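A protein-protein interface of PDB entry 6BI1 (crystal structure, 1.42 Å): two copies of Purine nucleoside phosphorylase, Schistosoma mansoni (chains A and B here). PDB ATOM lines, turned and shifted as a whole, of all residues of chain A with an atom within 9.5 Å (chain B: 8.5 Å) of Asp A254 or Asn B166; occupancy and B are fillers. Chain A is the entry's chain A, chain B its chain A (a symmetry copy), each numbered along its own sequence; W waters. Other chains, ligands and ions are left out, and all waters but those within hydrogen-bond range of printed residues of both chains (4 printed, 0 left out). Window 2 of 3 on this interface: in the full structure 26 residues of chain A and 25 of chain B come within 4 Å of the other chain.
The backbone carbonyl oxygen (O) of Ser A256 sits at hydrogen-bond distance from the side-chain amino group (NZ) of Lys A261, at 2.9 Å. O of Asp B163 sits at hydrogen-bond distance from SG of Cys B231 (3.7 Å). The side-chain carboxylate (OD1) of Asp B163 is in hydrogen-bond range of the backbone NH (N) of Ser B165 (3.0 Å).
Pro A205 touches Ser B165 (CG to CB, 3.96 Å). Asp A206 touches Gly B136 (OD2 to CA, 3.5 Å). Asp A254 touches Asn B166 (OD1 to ND2, 3.5 Å). CB of Ser A256 touches OD2 of Asp B163 (3.1 Å). Ile A257 touches Asp B163.
Of the printed residues of chain B, Pro A205 touches Ser B165 (3.96 Å). Printed residues of chain B within 4 Å of Asp A206: Gly B136 (3.5 Å). Asp A254 touches just one residue of chain B: Asn B166. Printed residues of chain B within 4 Å of Ser A256: Asp B163. Of chain A, only Pro A205 comes within 4 Å of Ser B165. Asn B166 touches one residue of chain A. Ala B167 touches none of the printed residues of chain A. The nearest residue of chain A that does not touch Asn B166 is Ser A256 (5.2 Å).
Hydrophobic or aromatic side chains of chain A within 4 Å of the printed part of chain B: Pro A205.
No position is printed for both chains. Of the 5 pairs that touch across the chains among the printed residues, none has its exchanged pair printed and touching as well.
Water W2 bridges NZ of Lys B135 (2.6 Å) and OD1 of Asp A206 (2.6 Å). Water W1 bridges N of Leu B164 (2.8 Å) and O of Glu A203 (3.1 Å). Water W4 lies within hydrogen-bond range of OD1 of Asp B163 and O of Glu A203. Water W3 lies within hydrogen-bond range of OD2 of Asp B163 and O of Ile A257.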
ATOM      1  N   GLU A 203     -11.431   0.565  12.116  1.00  0.00           N
ATOM      2  CA  GLU A 203     -11.446  -0.165  10.852  1.00  0.00           C
ATOM      3  C   GLU A 203     -10.092  -0.816  10.602  1.00  0.00           C
ATOM      4  O   GLU A 203      -9.038  -0.201  10.800  1.00  0.00           O
ATOM      5  CB  GLU A 203     -11.800   0.821   9.710  1.00  0.00           C
ATOM      6  CG  GLU A 203     -10.733   1.960   9.351  1.00  0.00           C
ATOM      7  CD  GLU A 203     -10.764   3.209  10.230  1.00  0.00           C
ATOM      8  OE1 GLU A 203      -9.994   4.185   9.961  1.00  0.00           O
ATOM      9  OE2 GLU A 203     -11.508   3.251  11.208  1.00  0.00           O
ATOM     10  N   SER A 204     -10.111  -2.101  10.201  1.00  0.00           N
ATOM     11  CA  SER A 204      -8.876  -2.799   9.881  1.00  0.00           C
ATOM     12  C   SER A 204      -8.291  -2.299   8.557  1.00  0.00           C
ATOM     13  O   SER A 204      -8.995  -1.685   7.760  1.00  0.00           O
ATOM     14  CB  SER A 204      -9.110  -4.306   9.782  1.00  0.00           C
ATOM     15  OG  SER A 204      -9.824  -4.603   8.591  1.00  0.00           O
ATOM     16  N   PRO A 205      -7.010  -2.563   8.304  1.00  0.00           N
ATOM     17  CA  PRO A 205      -6.414  -2.110   7.022  1.00  0.00           C
ATOM     18  C   PRO A 205      -7.185  -2.588   5.806  1.00  0.00           C
ATOM     19  O   PRO A 205      -7.403  -1.809   4.857  1.00  0.00           O
ATOM     20  CB  PRO A 205      -4.998  -2.682   7.073  1.00  0.00           C
ATOM     21  CG  PRO A 205      -4.685  -2.731   8.539  1.00  0.00           C
ATOM     22  CD  PRO A 205      -5.980  -3.055   9.239  1.00  0.00           C
ATOM     23  N   ASP A 206      -7.642  -3.849   5.820  1.00  0.00           N
ATOM     24  CA  ASP A 206      -8.402  -4.382   4.690  1.00  0.00           C
ATOM     25  C   ASP A 206      -9.822  -3.836   4.626  1.00  0.00           C
ATOM     26  O   ASP A 206     -10.374  -3.705   3.523  1.00  0.00           O
ATOM     27  CB  ASP A 206      -8.347  -5.909   4.677  1.00  0.00           C
ATOM     28  CG  ASP A 206      -6.932  -6.399   4.434  1.00  0.00           C
ATOM     29  OD1 ASP A 206      -6.407  -6.248   3.283  1.00  0.00           O
ATOM     30  OD2 ASP A 206      -6.292  -6.847   5.413  1.00  0.00           O
ATOM     31  N   ASN A 246      -5.125   9.455   7.946  1.00  0.00           N
ATOM     32  CA  ASN A 246      -5.555   8.813   6.699  1.00  0.00           C
ATOM     33  C   ASN A 246      -5.317   7.306   6.814  1.00  0.00           C
ATOM     34  O   ASN A 246      -4.171   6.836   6.804  1.00  0.00           O
ATOM     35  CB  ASN A 246      -4.874   9.412   5.456  1.00  0.00           C
ATOM     36  CG  ASN A 246      -5.507   8.909   4.178  1.00  0.00           C
ATOM     37  OD1 ASN A 246      -5.398   7.731   3.871  1.00  0.00           O
ATOM     38  ND2 ASN A 246      -6.220   9.790   3.443  1.00  0.00           N
ATOM     39  N   SER A 247      -6.414   6.534   6.916  1.00  0.00           N
ATOM     40  CA  SER A 247      -6.294   5.106   7.166  1.00  0.00           C
ATOM     41  C   SER A 247      -5.704   4.352   5.977  1.00  0.00           C
ATOM     42  O   SER A 247      -5.105   3.295   6.159  1.00  0.00           O
ATOM     43  CB  SER A 247      -7.666   4.488   7.519  1.00  0.00           C
ATOM     44  OG  SER A 247      -8.268   5.180   8.592  1.00  0.00           O
ATOM     45  N   ILE A 248      -5.867   4.881   4.754  1.00  0.00           N
ATOM     46  CA  ILE A 248      -5.308   4.227   3.572  1.00  0.00           C
ATOM     47  C   ILE A 248      -3.786   4.380   3.547  1.00  0.00           C
ATOM     48  O   ILE A 248      -3.054   3.405   3.326  1.00  0.00           O
ATOM     49  CB  ILE A 248      -5.996   4.767   2.297  1.00  0.00           C
ATOM     50  CG1 ILE A 248      -7.468   4.272   2.206  1.00  0.00           C
ATOM     51  CG2 ILE A 248      -5.203   4.393   1.025  1.00  0.00           C
ATOM     52  CD1 ILE A 248      -7.635   2.780   1.893  1.00  0.00           C
ATOM     53  N   LEU A 249      -3.281   5.600   3.805  1.00  0.00           N
ATOM     54  CA  LEU A 249      -1.831   5.799   3.913  1.00  0.00           C
ATOM     55  C   LEU A 249      -1.248   4.956   5.038  1.00  0.00           C
ATOM     56  O   LEU A 249      -0.195   4.328   4.867  1.00  0.00           O
ATOM     57  CB  LEU A 249      -1.477   7.284   4.112  1.00  0.00           C
ATOM     58  CG  LEU A 249      -1.547   8.218   2.898  1.00  0.00           C
ATOM     59  CD1 LEU A 249      -0.905   9.556   3.257  1.00  0.00           C
ATOM     60  CD2 LEU A 249      -0.861   7.646   1.685  1.00  0.00           C
ATOM     61  N   ASP A 250      -1.938   4.909   6.191  1.00  0.00           N
ATOM     62  CA  ASP A 250      -1.435   4.127   7.315  1.00  0.00           C
ATOM     63  C   ASP A 250      -1.346   2.646   6.952  1.00  0.00           C
ATOM     64  O   ASP A 250      -0.386   1.960   7.323  1.00  0.00           O
ATOM     65  CB  ASP A 250      -2.325   4.338   8.545  1.00  0.00           C
ATOM     66  CG  ASP A 250      -2.237   5.761   9.145  1.00  0.00           C
ATOM     67  OD1 ASP A 250      -1.390   6.586   8.721  1.00  0.00           O
ATOM     68  OD2 ASP A 250      -3.037   6.050  10.070  1.00  0.00           O
ATOM     69  N   ALA A 251      -2.322   2.143   6.198  1.00  0.00           N
ATOM     70  CA  ALA A 251      -2.279   0.739   5.775  1.00  0.00           C
ATOM     71  C   ALA A 251      -1.109   0.467   4.835  1.00  0.00           C
ATOM     72  O   ALA A 251      -0.415  -0.551   4.967  1.00  0.00           O
ATOM     73  CB  ALA A 251      -3.616   0.370   5.125  1.00  0.00           C
ATOM     74  N   GLU A 252      -0.839   1.392   3.905  1.00  0.00           N
ATOM     75  CA  GLU A 252       0.254   1.228   2.951  1.00  0.00           C
ATOM     76  C   GLU A 252       1.626   1.307   3.621  1.00  0.00           C
ATOM     77  O   GLU A 252       2.585   0.676   3.146  1.00  0.00           O
ATOM     78  CB  GLU A 252       0.103   2.275   1.834  1.00  0.00           C
ATOM     79  CG  GLU A 252      -1.140   1.991   0.958  1.00  0.00           C
ATOM     80  CD  GLU A 252      -1.409   3.002  -0.153  1.00  0.00           C
ATOM     81  OE1 GLU A 252      -1.010   4.173  -0.032  1.00  0.00           O
ATOM     82  OE2 GLU A 252      -2.053   2.613  -1.153  1.00  0.00           O
ATOM     83  N   ASN A 253       1.743   2.044   4.731  1.00  0.00           N
ATOM     84  CA  ASN A 253       3.006   2.207   5.442  1.00  0.00           C
ATOM     85  C   ASN A 253       3.126   1.373   6.717  1.00  0.00           C
ATOM     86  O   ASN A 253       4.162   1.453   7.386  1.00  0.00           O
ATOM     87  CB  ASN A 253       3.209   3.676   5.831  1.00  0.00           C
ATOM     88  CG  ASN A 253       3.364   4.589   4.647  1.00  0.00           C
ATOM     89  OD1 ASN A 253       4.205   4.381   3.768  1.00  0.00           O
ATOM     90  ND2 ASN A 253       2.608   5.683   4.667  1.00  0.00           N
ATOM     91  N   ASP A 254       2.106   0.588   7.073  1.00  0.00           N
ATOM     92  CA  ASP A 254       2.092  -0.211   8.307  1.00  0.00           C
ATOM     93  C   ASP A 254       2.255   0.643   9.573  1.00  0.00           C
ATOM     94  O   ASP A 254       3.066   0.333  10.453  1.00  0.00           O
ATOM     95  CB  ASP A 254       3.116  -1.349   8.264  1.00  0.00           C
ATOM     96  CG  ASP A 254       2.868  -2.384   9.345  1.00  0.00           C
ATOM     97  OD1 ASP A 254       1.764  -2.373   9.939  1.00  0.00           O
ATOM     98  OD2 ASP A 254       3.774  -3.205   9.601  1.00  0.00           O
ATOM     99  N   VAL A 255       1.444   1.703   9.669  1.00  0.00           N
ATOM    100  CA  VAL A 255       1.431   2.650  10.788  1.00  0.00           C
ATOM    101  C   VAL A 255       0.128   2.502  11.576  1.00  0.00           C
ATOM    102  O   VAL A 255      -0.953   2.351  10.993  1.00  0.00           O
ATOM    103  CB  VAL A 255       1.576   4.099  10.269  1.00  0.00           C
ATOM    104  CG1 VAL A 255       1.118   5.129  11.334  1.00  0.00           C
ATOM    105  CG2 VAL A 255       2.993   4.355   9.813  1.00  0.00           C
ATOM    106  N   SER A 256       0.227   2.608  12.903  1.00  0.00           N
ATOM    107  CA  SER A 256      -0.877   2.325  13.813  1.00  0.00           C
ATOM    108  C   SER A 256      -1.636   3.595  14.192  1.00  0.00           C
ATOM    109  O   SER A 256      -1.172   4.717  14.003  1.00  0.00           O
ATOM    110  CB  SER A 256      -0.345   1.674  15.086  1.00  0.00           C
ATOM    111  OG  SER A 256       0.197   2.659  15.952  1.00  0.00           O
ATOM    112  N   ILE A 257      -2.822   3.396  14.761  1.00  0.00           N
ATOM    113  CA  ILE A 257      -3.661   4.489  15.234  1.00  0.00           C
ATOM    114  C   ILE A 257      -4.110   4.141  16.642  1.00  0.00           C
ATOM    115  O   ILE A 257      -4.313   2.971  16.979  1.00  0.00           O
ATOM    116  CB  ILE A 257      -4.874   4.732  14.306  1.00  0.00           C
ATOM    117  CG1 ILE A 257      -5.709   5.941  14.766  1.00  0.00           C
ATOM    118  CG2 ILE A 257      -5.733   3.487  14.238  1.00  0.00           C
ATOM    119  CD1 ILE A 257      -5.028   7.309  14.553  1.00  0.00           C
ATOM    120  N   LYS A 261      -3.460   9.487  19.894  1.00  0.00           N
ATOM    121  CA  LYS A 261      -3.206  10.300  18.706  1.00  0.00           C
ATOM    122  C   LYS A 261      -4.460  11.060  18.283  1.00  0.00           C
ATOM    123  O   LYS A 261      -4.377  12.215  17.847  1.00  0.00           O
ATOM    124  CB  LYS A 261      -2.714   9.427  17.548  1.00  0.00           C
ATOM    125  CG  LYS A 261      -1.301   8.866  17.687  1.00  0.00           C
ATOM    126  CD  LYS A 261      -0.987   7.962  16.486  1.00  0.00           C
ATOM    127  CE  LYS A 261       0.308   7.184  16.666  1.00  0.00           C
ATOM    128  NZ  LYS A 261       0.662   6.417  15.433  1.00  0.00           N
ATOM    129  N   LYS B 135      -3.792 -12.952   6.912  1.00  0.00           N
ATOM    130  CA  LYS B 135      -2.986 -11.749   7.141  1.00  0.00           C
ATOM    131  C   LYS B 135      -3.825 -10.510   7.459  1.00  0.00           C
ATOM    132  O   LYS B 135      -3.245  -9.459   7.784  1.00  0.00           O
ATOM    133  CB  LYS B 135      -2.074 -11.457   5.942  1.00  0.00           C
ATOM    134  CG  LYS B 135      -2.810 -11.034   4.693  1.00  0.00           C
ATOM    135  CD  LYS B 135      -1.809 -10.924   3.526  1.00  0.00           C
ATOM    136  CE  LYS B 135      -2.504 -10.645   2.200  1.00  0.00           C
ATOM    137  NZ  LYS B 135      -3.158  -9.306   2.195  1.00  0.00           N
ATOM    138  N   GLY B 136      -5.148 -10.596   7.357  1.00  0.00           N
ATOM    139  CA  GLY B 136      -6.059  -9.500   7.653  1.00  0.00           C
ATOM    140  C   GLY B 136      -7.488  -9.991   7.477  1.00  0.00           C
ATOM    141  O   GLY B 136      -7.725 -11.143   7.062  1.00  0.00           O
ATOM    142  N   ASP B 163      -6.680  -1.136  18.079  1.00  0.00           N
ATOM    143  CA  ASP B 163      -6.132  -1.148  16.722  1.00  0.00           C
ATOM    144  C   ASP B 163      -5.831  -2.592  16.333  1.00  0.00           C
ATOM    145  O   ASP B 163      -5.124  -3.296  17.062  1.00  0.00           O
ATOM    146  CB  ASP B 163      -4.837  -0.327  16.723  1.00  0.00           C
ATOM    147  CG  ASP B 163      -4.040  -0.429  15.423  1.00  0.00           C
ATOM    148  OD1 ASP B 163      -4.610  -0.725  14.362  1.00  0.00           O
ATOM    149  OD2 ASP B 163      -2.818  -0.158  15.482  1.00  0.00           O
ATOM    150  N   LEU B 164      -6.370  -3.034  15.194  1.00  0.00           N
ATOM    151  CA  LEU B 164      -6.201  -4.412  14.739  1.00  0.00           C
ATOM    152  C   LEU B 164      -5.139  -4.556  13.648  1.00  0.00           C
ATOM    153  O   LEU B 164      -5.050  -5.628  13.028  1.00  0.00           O
ATOM    154  CB  LEU B 164      -7.539  -4.965  14.218  1.00  0.00           C
ATOM    155  CG  LEU B 164      -8.727  -4.865  15.175  1.00  0.00           C
ATOM    156  CD1 LEU B 164     -10.029  -5.335  14.508  1.00  0.00           C
ATOM    157  CD2 LEU B 164      -8.462  -5.609  16.489  1.00  0.00           C
ATOM    158  N   SER B 165      -4.355  -3.508  13.375  1.00  0.00           N
ATOM    159  CA  SER B 165      -3.439  -3.563  12.244  1.00  0.00           C
ATOM    160  C   SER B 165      -2.362  -4.632  12.390  1.00  0.00           C
ATOM    161  O   SER B 165      -1.808  -5.067  11.370  1.00  0.00           O
ATOM    162  CB  SER B 165      -2.839  -2.179  11.994  1.00  0.00           C
ATOM    163  OG  SER B 165      -2.016  -1.788  13.073  1.00  0.00           O
ATOM    164  N   ASN B 166      -2.023  -5.053  13.619  1.00  0.00           N
ATOM    165  CA  ASN B 166      -1.053  -6.125  13.859  1.00  0.00           C
ATOM    166  C   ASN B 166      -1.688  -7.322  14.578  1.00  0.00           C
ATOM    167  O   ASN B 166      -1.014  -8.052  15.311  1.00  0.00           O
ATOM    168  CB  ASN B 166       0.177  -5.583  14.593  1.00  0.00           C
ATOM    169  CG  ASN B 166       0.803  -4.392  13.862  1.00  0.00           C
ATOM    170  OD1 ASN B 166       0.886  -3.287  14.402  1.00  0.00           O
ATOM    171  ND2 ASN B 166       1.220  -4.613  12.618  1.00  0.00           N
ATOM    172  N   ALA B 167      -2.978  -7.569  14.328  1.00  0.00           N
ATOM    173  CA  ALA B 167      -3.676  -8.681  14.979  1.00  0.00           C
ATOM    174  C   ALA B 167      -3.105 -10.037  14.588  1.00  0.00           C
ATOM    175  O   ALA B 167      -3.106 -10.960  15.416  1.00  0.00           O
ATOM    176  CB  ALA B 167      -5.168  -8.622  14.660  1.00  0.00           C
ATOM    177  N   TYR B 168      -2.620 -10.181  13.343  1.00  0.00           N
ATOM    178  CA  TYR B 168      -2.070 -11.437  12.809  1.00  0.00           C
ATOM    179  C   TYR B 168      -0.549 -11.285  12.754  1.00  0.00           C
ATOM    180  O   TYR B 168      -0.008 -10.688  11.820  1.00  0.00           O
ATOM    181  CB  TYR B 168      -2.691 -11.749  11.433  1.00  0.00           C
ATOM    182  CG  TYR B 168      -4.218 -11.875  11.463  1.00  0.00           C
ATOM    183  CD1 TYR B 168      -4.842 -13.056  11.824  1.00  0.00           C
ATOM    184  CD2 TYR B 168      -5.052 -10.768  11.190  1.00  0.00           C
ATOM    185  CE1 TYR B 168      -6.244 -13.160  11.894  1.00  0.00           C
ATOM    186  CE2 TYR B 168      -6.436 -10.869  11.233  1.00  0.00           C
ATOM    187  CZ  TYR B 168      -7.048 -12.074  11.592  1.00  0.00           C
ATOM    188  OH  TYR B 168      -8.422 -12.205  11.672  1.00  0.00           O
ATOM    189  N   ASP B 169       0.142 -11.882  13.734  1.00  0.00           N
ATOM    190  CA  ASP B 169       1.587 -11.691  13.893  1.00  0.00           C
ATOM    191  C   ASP B 169       2.363 -12.123  12.646  1.00  0.00           C
ATOM    192  O   ASP B 169       2.228 -13.258  12.171  1.00  0.00           O
ATOM    193  CB  ASP B 169       2.072 -12.490  15.114  1.00  0.00           C
ATOM    194  CG  ASP B 169       3.543 -12.230  15.455  1.00  0.00           C
ATOM    195  OD1 ASP B 169       3.816 -11.241  16.167  1.00  0.00           O
ATOM    196  OD2 ASP B 169       4.420 -13.009  15.021  1.00  0.00           O
ATOM    197  N   ARG B 170       3.239 -11.236  12.153  1.00  0.00           N
ATOM    198  CA  ARG B 170       3.970 -11.511  10.915  1.00  0.00           C
ATOM    199  C   ARG B 170       5.027 -12.609  11.082  1.00  0.00           C
ATOM    200  O   ARG B 170       5.226 -13.423  10.171  1.00  0.00           O
ATOM    201  CB  ARG B 170       4.622 -10.224  10.406  1.00  0.00           C
ATOM    202  N   GLN B 173       3.446 -16.115  10.980  1.00  0.00           N
ATOM    203  CA  GLN B 173       3.181 -16.492   9.590  1.00  0.00           C
ATOM    204  C   GLN B 173       4.459 -16.974   8.905  1.00  0.00           C
ATOM    205  O   GLN B 173       4.450 -17.980   8.184  1.00  0.00           O
ATOM    206  CB  GLN B 173       2.580 -15.304   8.829  1.00  0.00           C
ATOM    207  CG  GLN B 173       1.166 -14.886   9.248  1.00  0.00           C
ATOM    208  CD  GLN B 173       0.725 -13.584   8.577  1.00  0.00           C
ATOM    209  OE1 GLN B 173       0.769 -13.456   7.350  1.00  0.00           O
ATOM    210  NE2 GLN B 173       0.312 -12.617   9.377  1.00  0.00           N
ATOM    211  N   VAL B 227     -10.037 -13.638  17.522  1.00  0.00           N
ATOM    212  CA  VAL B 227      -8.884 -12.794  17.185  1.00  0.00           C
ATOM    213  C   VAL B 227      -9.003 -11.428  17.853  1.00  0.00           C
ATOM    214  O   VAL B 227      -8.010 -10.890  18.390  1.00  0.00           O
ATOM    215  CB  VAL B 227      -8.734 -12.648  15.655  1.00  0.00           C
ATOM    216  CG1 VAL B 227      -7.688 -11.580  15.264  1.00  0.00           C
ATOM    217  CG2 VAL B 227      -8.374 -13.965  15.018  1.00  0.00           C
ATOM    218  N   CYS B 231      -6.433  -9.898  20.546  1.00  0.00           N
ATOM    219  CA  CYS B 231      -5.693  -8.662  20.257  1.00  0.00           C
ATOM    220  C   CYS B 231      -5.949  -7.598  21.331  1.00  0.00           C
ATOM    221  O   CYS B 231      -5.017  -6.924  21.790  1.00  0.00           O
ATOM    222  CB  CYS B 231      -6.109  -8.150  18.867  1.00  0.00           C
ATOM    223  SG  CYS B 231      -5.150  -6.745  18.263  1.00  0.00           S
ATOM    224  N   ILE B 235      -2.610 -10.856  23.300  1.00  0.00           N
ATOM    225  CA  ILE B 235      -2.187 -12.204  22.905  1.00  0.00           C
ATOM    226  C   ILE B 235      -1.915 -12.211  21.400  1.00  0.00           C
ATOM    227  O   ILE B 235      -2.755 -11.757  20.617  1.00  0.00           O
ATOM    228  CB  ILE B 235      -3.274 -13.231  23.287  1.00  0.00           C
ATOM    229  CG1 ILE B 235      -3.439 -13.326  24.828  1.00  0.00           C
ATOM    230  CG2 ILE B 235      -3.000 -14.559  22.671  1.00  0.00           C
ATOM    231  CD1 ILE B 235      -4.594 -14.199  25.294  1.00  0.00           C
ATOM    232  N   LYS B 236      -0.751 -12.731  20.991  1.00  0.00           N
ATOM    233  CA  LYS B 236      -0.392 -12.864  19.571  1.00  0.00           C
ATOM    234  C   LYS B 236      -1.181 -14.018  18.948  1.00  0.00           C
ATOM    235  O   LYS B 236      -1.469 -15.020  19.617  1.00  0.00           O
ATOM    236  CB  LYS B 236       1.101 -13.176  19.442  1.00  0.00           C
ATOM    237  CG  LYS B 236       2.031 -12.112  19.973  1.00  0.00           C
ATOM    238  CD  LYS B 236       3.493 -12.594  19.846  1.00  0.00           C
ATOM    239  CE  LYS B 236       4.479 -11.461  19.982  1.00  0.00           C
ATOM    240  NZ  LYS B 236       5.888 -11.969  19.934  1.00  0.00           N
ATOM    241  N   VAL B 237      -1.508 -13.890  17.652  1.00  0.00           N
ATOM    242  CA  VAL B 237      -2.369 -14.859  16.961  1.00  0.00           C
ATOM    243  C   VAL B 237      -1.740 -15.331  15.653  1.00  0.00           C
ATOM    244  O   VAL B 237      -1.192 -14.527  14.889  1.00  0.00           O
ATOM    245  CB  VAL B 237      -3.735 -14.230  16.639  1.00  0.00           C
ATOM    246  CG1 VAL B 237      -4.566 -15.157  15.744  1.00  0.00           C
ATOM    247  CG2 VAL B 237      -4.503 -13.939  17.911  1.00  0.00           C
HETATM  248  O   HOH W   1      -7.869  -1.715  13.213  1.00  0.00           O
HETATM  249  O   HOH W   2      -4.406  -7.093   1.793  1.00  0.00           O
HETATM  250  O   HOH W   3      -2.033   0.915  18.527  1.00  0.00           O
HETATM  251  O   HOH W   4      -6.001   0.060  12.038  1.00  0.00           O
